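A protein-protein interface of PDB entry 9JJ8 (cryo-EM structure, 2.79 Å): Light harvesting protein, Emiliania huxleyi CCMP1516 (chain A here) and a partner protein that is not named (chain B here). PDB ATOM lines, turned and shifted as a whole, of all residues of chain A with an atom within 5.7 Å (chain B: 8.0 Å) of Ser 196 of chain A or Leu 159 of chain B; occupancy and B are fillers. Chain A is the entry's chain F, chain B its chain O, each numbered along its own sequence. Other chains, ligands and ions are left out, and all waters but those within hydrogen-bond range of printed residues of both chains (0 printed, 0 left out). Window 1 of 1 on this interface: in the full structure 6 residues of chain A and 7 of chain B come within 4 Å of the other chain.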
ATOM      1  N   PHE A 194      29.022  22.456  -0.454  1.00  0.00           N
ATOM      2  CA  PHE A 194      29.765  21.459   0.302  1.00  0.00           C
ATOM      3  C   PHE A 194      28.844  20.468   0.999  1.00  0.00           C
ATOM      4  O   PHE A 194      29.224  19.309   1.194  1.00  0.00           O
ATOM      5  CB  PHE A 194      30.667  22.153   1.330  1.00  0.00           C
ATOM      6  CG  PHE A 194      31.481  21.210   2.173  1.00  0.00           C
ATOM      7  CD1 PHE A 194      32.654  20.669   1.682  1.00  0.00           C
ATOM      8  CD2 PHE A 194      31.088  20.888   3.465  1.00  0.00           C
ATOM      9  CE1 PHE A 194      33.412  19.814   2.452  1.00  0.00           C
ATOM     10  CE2 PHE A 194      31.843  20.027   4.240  1.00  0.00           C
ATOM     11  CZ  PHE A 194      33.008  19.490   3.731  1.00  0.00           C
ATOM     12  N   LEU A 195      27.643  20.901   1.372  1.00  0.00           N
ATOM     13  CA  LEU A 195      26.666  20.020   1.987  1.00  0.00           C
ATOM     14  C   LEU A 195      25.992  19.156   0.923  1.00  0.00           C
ATOM     15  O   LEU A 195      26.172  19.351  -0.282  1.00  0.00           O
ATOM     16  CB  LEU A 195      25.628  20.824   2.776  1.00  0.00           C
ATOM     17  CG  LEU A 195      24.511  21.615   2.084  1.00  0.00           C
ATOM     18  CD1 LEU A 195      23.430  21.957   3.095  1.00  0.00           C
ATOM     19  CD2 LEU A 195      25.017  22.890   1.427  1.00  0.00           C
ATOM     20  N   SER A 196      25.214  18.181   1.388  1.00  0.00           N
ATOM     21  CA  SER A 196      24.603  17.208   0.493  1.00  0.00           C
ATOM     22  C   SER A 196      23.523  17.856  -0.367  1.00  0.00           C
ATOM     23  O   SER A 196      22.850  18.805   0.044  1.00  0.00           O
ATOM     24  CB  SER A 196      24.013  16.051   1.297  1.00  0.00           C
ATOM     25  OG  SER A 196      24.917  15.614   2.295  1.00  0.00           O
ATOM     26  N   LYS A 197      23.361  17.328  -1.581  1.00  0.00           N
ATOM     27  CA  LYS A 197      22.486  17.927  -2.580  1.00  0.00           C
ATOM     28  C   LYS A 197      21.044  17.442  -2.503  1.00  0.00           C
ATOM     29  O   LYS A 197      20.198  17.956  -3.243  1.00  0.00           O
ATOM     30  CB  LYS A 197      23.037  17.662  -3.986  1.00  0.00           C
ATOM     31  CG  LYS A 197      24.404  18.280  -4.243  1.00  0.00           C
ATOM     32  CD  LYS A 197      24.447  19.736  -3.801  1.00  0.00           C
ATOM     33  CE  LYS A 197      25.830  20.335  -3.989  1.00  0.00           C
ATOM     34  NZ  LYS A 197      26.222  20.384  -5.424  1.00  0.00           N
ATOM     35  N   ASP A 198      20.738  16.476  -1.644  1.00  0.00           N
ATOM     36  CA  ASP A 198      19.357  16.061  -1.434  1.00  0.00           C
ATOM     37  C   ASP A 198      18.718  16.966  -0.380  1.00  0.00           C
ATOM     38  O   ASP A 198      19.269  17.999   0.006  1.00  0.00           O
ATOM     39  CB  ASP A 198      19.290  14.589  -1.043  1.00  0.00           C
ATOM     40  CG  ASP A 198      20.061  14.295   0.218  1.00  0.00           C
ATOM     41  OD1 ASP A 198      21.026  15.032   0.496  1.00  0.00           O
ATOM     42  OD2 ASP A 198      19.690  13.347   0.939  1.00  0.00           O
ATOM     43  N   ALA A 201      19.259  14.966   3.992  1.00  0.00           N
ATOM     44  CA  ALA A 201      20.600  15.079   4.559  1.00  0.00           C
ATOM     45  C   ALA A 201      20.980  16.531   4.814  1.00  0.00           C
ATOM     46  O   ALA A 201      21.609  16.843   5.831  1.00  0.00           O
ATOM     47  CB  ALA A 201      21.612  14.421   3.630  1.00  0.00           C
ATOM     48  N   ALA A 202      20.609  17.429   3.896  1.00  0.00           N
ATOM     49  CA  ALA A 202      20.885  18.849   4.089  1.00  0.00           C
ATOM     50  C   ALA A 202      20.128  19.400   5.291  1.00  0.00           C
ATOM     51  O   ALA A 202      20.686  20.163   6.089  1.00  0.00           O
ATOM     52  CB  ALA A 202      20.526  19.627   2.823  1.00  0.00           C
ATOM     53  N   LYS A 208      21.641  19.863  12.839  1.00  0.00           N
ATOM     54  CA  LYS A 208      22.842  19.674  13.648  1.00  0.00           C
ATOM     55  C   LYS A 208      23.507  21.010  13.961  1.00  0.00           C
ATOM     56  O   LYS A 208      23.904  21.268  15.107  1.00  0.00           O
ATOM     57  CB  LYS A 208      23.819  18.757  12.913  1.00  0.00           C
ATOM     58  CG  LYS A 208      23.438  17.287  12.906  1.00  0.00           C
ATOM     59  CD  LYS A 208      23.953  16.574  11.662  1.00  0.00           C
ATOM     60  CE  LYS A 208      24.250  15.110  11.942  1.00  0.00           C
ATOM     61  NZ  LYS A 208      24.983  14.465  10.819  1.00  0.00           N
ATOM     62  N   LEU B  80      22.497   4.143  11.495  1.00  0.00           N
ATOM     63  CA  LEU B  80      23.320   5.100  10.774  1.00  0.00           C
ATOM     64  C   LEU B  80      23.923   4.339   9.602  1.00  0.00           C
ATOM     65  O   LEU B  80      24.279   3.164   9.755  1.00  0.00           O
ATOM     66  CB  LEU B  80      24.397   5.694  11.705  1.00  0.00           C
ATOM     67  CG  LEU B  80      25.099   7.026  11.418  1.00  0.00           C
ATOM     68  CD1 LEU B  80      24.069   8.140  11.383  1.00  0.00           C
ATOM     69  CD2 LEU B  80      26.122   7.339  12.489  1.00  0.00           C
ATOM     70  N   PRO B  81      24.020   4.964   8.417  1.00  0.00           N
ATOM     71  CA  PRO B  81      24.175   4.196   7.167  1.00  0.00           C
ATOM     72  C   PRO B  81      25.439   3.346   7.105  1.00  0.00           C
ATOM     73  O   PRO B  81      26.496   3.724   7.615  1.00  0.00           O
ATOM     74  CB  PRO B  81      24.188   5.281   6.082  1.00  0.00           C
ATOM     75  CG  PRO B  81      24.428   6.565   6.799  1.00  0.00           C
ATOM     76  CD  PRO B  81      23.804   6.391   8.138  1.00  0.00           C
ATOM     77  N   GLU B  83      27.438   2.572   4.779  1.00  0.00           N
ATOM     78  CA  GLU B  83      28.587   3.084   4.040  1.00  0.00           C
ATOM     79  C   GLU B  83      29.520   3.862   4.959  1.00  0.00           C
ATOM     80  O   GLU B  83      30.740   3.650   4.956  1.00  0.00           O
ATOM     81  CB  GLU B  83      28.100   3.970   2.899  1.00  0.00           C
ATOM     82  CG  GLU B  83      26.921   3.407   2.121  1.00  0.00           C
ATOM     83  CD  GLU B  83      27.321   2.324   1.146  1.00  0.00           C
ATOM     84  OE1 GLU B  83      28.454   2.385   0.630  1.00  0.00           O
ATOM     85  OE2 GLU B  83      26.504   1.414   0.894  1.00  0.00           O
ATOM     86  N   TRP B  84      28.954   4.770   5.759  1.00  0.00           N
ATOM     87  CA  TRP B  84      29.746   5.517   6.729  1.00  0.00           C
ATOM     88  C   TRP B  84      30.292   4.596   7.812  1.00  0.00           C
ATOM     89  O   TRP B  84      31.402   4.810   8.308  1.00  0.00           O
ATOM     90  CB  TRP B  84      28.901   6.641   7.332  1.00  0.00           C
ATOM     91  CG  TRP B  84      29.550   7.405   8.454  1.00  0.00           C
ATOM     92  CD1 TRP B  84      29.527   7.097   9.783  1.00  0.00           C
ATOM     93  CD2 TRP B  84      30.304   8.619   8.341  1.00  0.00           C
ATOM     94  NE1 TRP B  84      30.225   8.035  10.501  1.00  0.00           N
ATOM     95  CE2 TRP B  84      30.711   8.982   9.640  1.00  0.00           C
ATOM     96  CE3 TRP B  84      30.678   9.432   7.267  1.00  0.00           C
ATOM     97  CZ2 TRP B  84      31.470  10.120   9.893  1.00  0.00           C
ATOM     98  CZ3 TRP B  84      31.433  10.562   7.522  1.00  0.00           C
ATOM     99  CH2 TRP B  84      31.818  10.896   8.823  1.00  0.00           C
ATOM    100  N   ILE B 155      34.411  12.831   1.861  1.00  0.00           N
ATOM    101  CA  ILE B 155      33.575  11.870   2.575  1.00  0.00           C
ATOM    102  C   ILE B 155      32.320  12.534   3.138  1.00  0.00           C
ATOM    103  O   ILE B 155      31.203  12.155   2.789  1.00  0.00           O
ATOM    104  CB  ILE B 155      34.378  11.151   3.682  1.00  0.00           C
ATOM    105  CG1 ILE B 155      35.400  10.198   3.062  1.00  0.00           C
ATOM    106  CG2 ILE B 155      33.451  10.367   4.586  1.00  0.00           C
ATOM    107  CD1 ILE B 155      36.548   9.849   3.986  1.00  0.00           C
ATOM    108  N   ALA B 156      32.485  13.539   4.004  1.00  0.00           N
ATOM    109  CA  ALA B 156      31.352  14.188   4.645  1.00  0.00           C
ATOM    110  C   ALA B 156      30.583  15.112   3.712  1.00  0.00           C
ATOM    111  O   ALA B 156      29.585  15.696   4.148  1.00  0.00           O
ATOM    112  CB  ALA B 156      31.822  14.975   5.871  1.00  0.00           C
ATOM    113  N   SER B 157      31.016  15.279   2.454  1.00  0.00           N
ATOM    114  CA  SER B 157      30.116  15.868   1.469  1.00  0.00           C
ATOM    115  C   SER B 157      28.884  14.995   1.250  1.00  0.00           C
ATOM    116  O   SER B 157      27.812  15.508   0.908  1.00  0.00           O
ATOM    117  CB  SER B 157      30.850  16.091   0.147  1.00  0.00           C
ATOM    118  OG  SER B 157      30.028  16.779  -0.779  1.00  0.00           O
ATOM    119  N   THR B 158      29.015  13.683   1.447  1.00  0.00           N
ATOM    120  CA  THR B 158      27.931  12.724   1.249  1.00  0.00           C
ATOM    121  C   THR B 158      27.712  11.938   2.537  1.00  0.00           C
ATOM    122  O   THR B 158      28.589  11.180   2.965  1.00  0.00           O
ATOM    123  CB  THR B 158      28.249  11.786   0.082  1.00  0.00           C
ATOM    124  OG1 THR B 158      29.495  11.122   0.331  1.00  0.00           O
ATOM    125  CG2 THR B 158      28.345  12.558  -1.227  1.00  0.00           C
ATOM    126  N   LEU B 159      26.541  12.108   3.151  1.00  0.00           N
ATOM    127  CA  LEU B 159      26.193  11.417   4.386  1.00  0.00           C
ATOM    128  C   LEU B 159      24.681  11.472   4.539  1.00  0.00           C
ATOM    129  O   LEU B 159      24.082  12.519   4.287  1.00  0.00           O
ATOM    130  CB  LEU B 159      26.870  12.066   5.604  1.00  0.00           C
ATOM    131  CG  LEU B 159      27.054  11.320   6.933  1.00  0.00           C
ATOM    132  CD1 LEU B 159      28.168  11.978   7.722  1.00  0.00           C
ATOM    133  CD2 LEU B 159      25.792  11.268   7.785  1.00  0.00           C
ATOM    134  N   ASN B 160      24.083  10.350   4.962  1.00  0.00           N
ATOM    135  CA  ASN B 160      22.647  10.257   5.272  1.00  0.00           C
ATOM    136  C   ASN B 160      21.778  10.663   4.084  1.00  0.00           C
ATOM    137  O   ASN B 160      20.733  11.299   4.239  1.00  0.00           O
ATOM    138  CB  ASN B 160      22.291  11.096   6.504  1.00  0.00           C
ATOM    139  CG  ASN B 160      22.280  10.287   7.783  1.00  0.00           C
ATOM    140  OD1 ASN B 160      22.066   9.077   7.762  1.00  0.00           O
ATOM    141  ND2 ASN B 160      22.510  10.954   8.908  1.00  0.00           N
ATOM    142  N   GLY B 161      22.199  10.277   2.884  1.00  0.00           N
ATOM    143  CA  GLY B 161      21.615  10.858   1.693  1.00  0.00           C
ATOM    144  C   GLY B 161      22.330  10.487   0.414  1.00  0.00           C
ATOM    145  O   GLY B 161      22.470   9.298   0.107  1.00  0.00           O
ATOM    146  N   GLY B 162      22.725  11.508  -0.357  1.00  0.00           N
ATOM    147  CA  GLY B 162      23.439  11.390  -1.620  1.00  0.00           C
ATOM    148  C   GLY B 162      24.547  10.357  -1.643  1.00  0.00           C
ATOM    149  O   GLY B 162      25.213  10.139  -0.625  1.00  0.00           O
ATOM    150  N   ASP B 163      24.751   9.736  -2.806  1.00  0.00           N
ATOM    151  CA  ASP B 163      25.369   8.416  -2.883  1.00  0.00           C
ATOM    152  C   ASP B 163      26.806   8.399  -2.372  1.00  0.00           C
ATOM    153  O   ASP B 163      27.541   9.385  -2.467  1.00  0.00           O
ATOM    154  CB  ASP B 163      25.311   7.882  -4.320  1.00  0.00           C
ATOM    155  CG  ASP B 163      25.977   8.805  -5.334  1.00  0.00           C
ATOM    156  OD1 ASP B 163      26.390   9.927  -4.975  1.00  0.00           O
ATOM    157  OD2 ASP B 163      26.090   8.395  -6.508  1.00  0.00           O
ATOM    158  N   ARG B 164      27.178   7.260  -1.798  1.00  0.00           N
ATOM    159  CA  ARG B 164      28.512   6.992  -1.274  1.00  0.00           C
ATOM    160  C   ARG B 164      29.337   6.185  -2.264  1.00  0.00           C
ATOM    161  O   ARG B 164      30.010   5.229  -1.883  1.00  0.00           O
ATOM    162  CB  ARG B 164      28.419   6.272   0.065  1.00  0.00           C
ATOM    163  CG  ARG B 164      27.721   7.070   1.148  1.00  0.00           C
ATOM    164  CD  ARG B 164      28.513   8.304   1.489  1.00  0.00           C
ATOM    165  NE  ARG B 164      29.855   7.996   1.970  1.00  0.00           N
ATOM    166  CZ  ARG B 164      30.174   7.822   3.245  1.00  0.00           C
ATOM    167  NH1 ARG B 164      29.272   7.932   4.204  1.00  0.00           N
ATOM    168  NH2 ARG B 164      31.435   7.541   3.565  1.00  0.00           N
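The side-chain hydroxyl (OG) of Ser 157 of chain B sits at hydrogen-bond distance from the backbone carbonyl oxygen (O) of Phe 194 of chain A (3.3 Å). The side-chain hydroxyl (OG) of Ser 196 of chain A sits at hydrogen-bond distance from the backbone carbonyl oxygen (O) of Ser 157 of chain B, 3.2 Å away.
Of the 8 printed residues of chain A, 4 touch a printed residue of chain B. Among the printed residues, no Asp or Glu carboxylate lies within 4 Å of a Lys or Arg side-chain nitrogen of the other chain.
The backbone NH of Ala 201 of chain A lies close to the side-chain carboxylate of Asp 198 of chain A, 3.5 Å away.
Of chain B, only Ser 157 (3.2 Å) and Leu 159 (3.8 Å) come within 4 Å of Ser 196 of chain A. Printed residues of chain A within 4 Å of Leu 159 of chain B: Ser 196 (3.8 Å) and Ala 201 (3.2 Å). Of the printed residues of chain A, Ser 157 of chain B touches Phe 194 and Ser 196. Of the printed residues of chain A, Gly 161 of chain B touches Asp 198 (3.2 Å). Of the printed residues of chain B, Ala 201 of chain A touches Leu 159 (3.2 Å) and Asn 160 (3.3 Å). Lys 208 of chain A touches none of the printed residues of chain B. Arg 164 of chain B touches none of the printed residues of chain A. The nearest printed residue of chain B that does not touch Asp 198 of chain A is Asn 160 of chain B (4.02 Å).
Among the printed residues, pairs that only touch across the chains: Ser 196 of chain A with Leu 159 of chain B (3.8 Å), Asp 198 of chain A with Gly 161 of chain B (3.2 Å), Asp 198 of chain A with Gly 162 of chain B (3.8 Å), Ala 201 of chain A with Leu 159 of chain B (3.2 Å) and Ala 201 of chain A with Asn 160 of chain B (3.3 Å).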
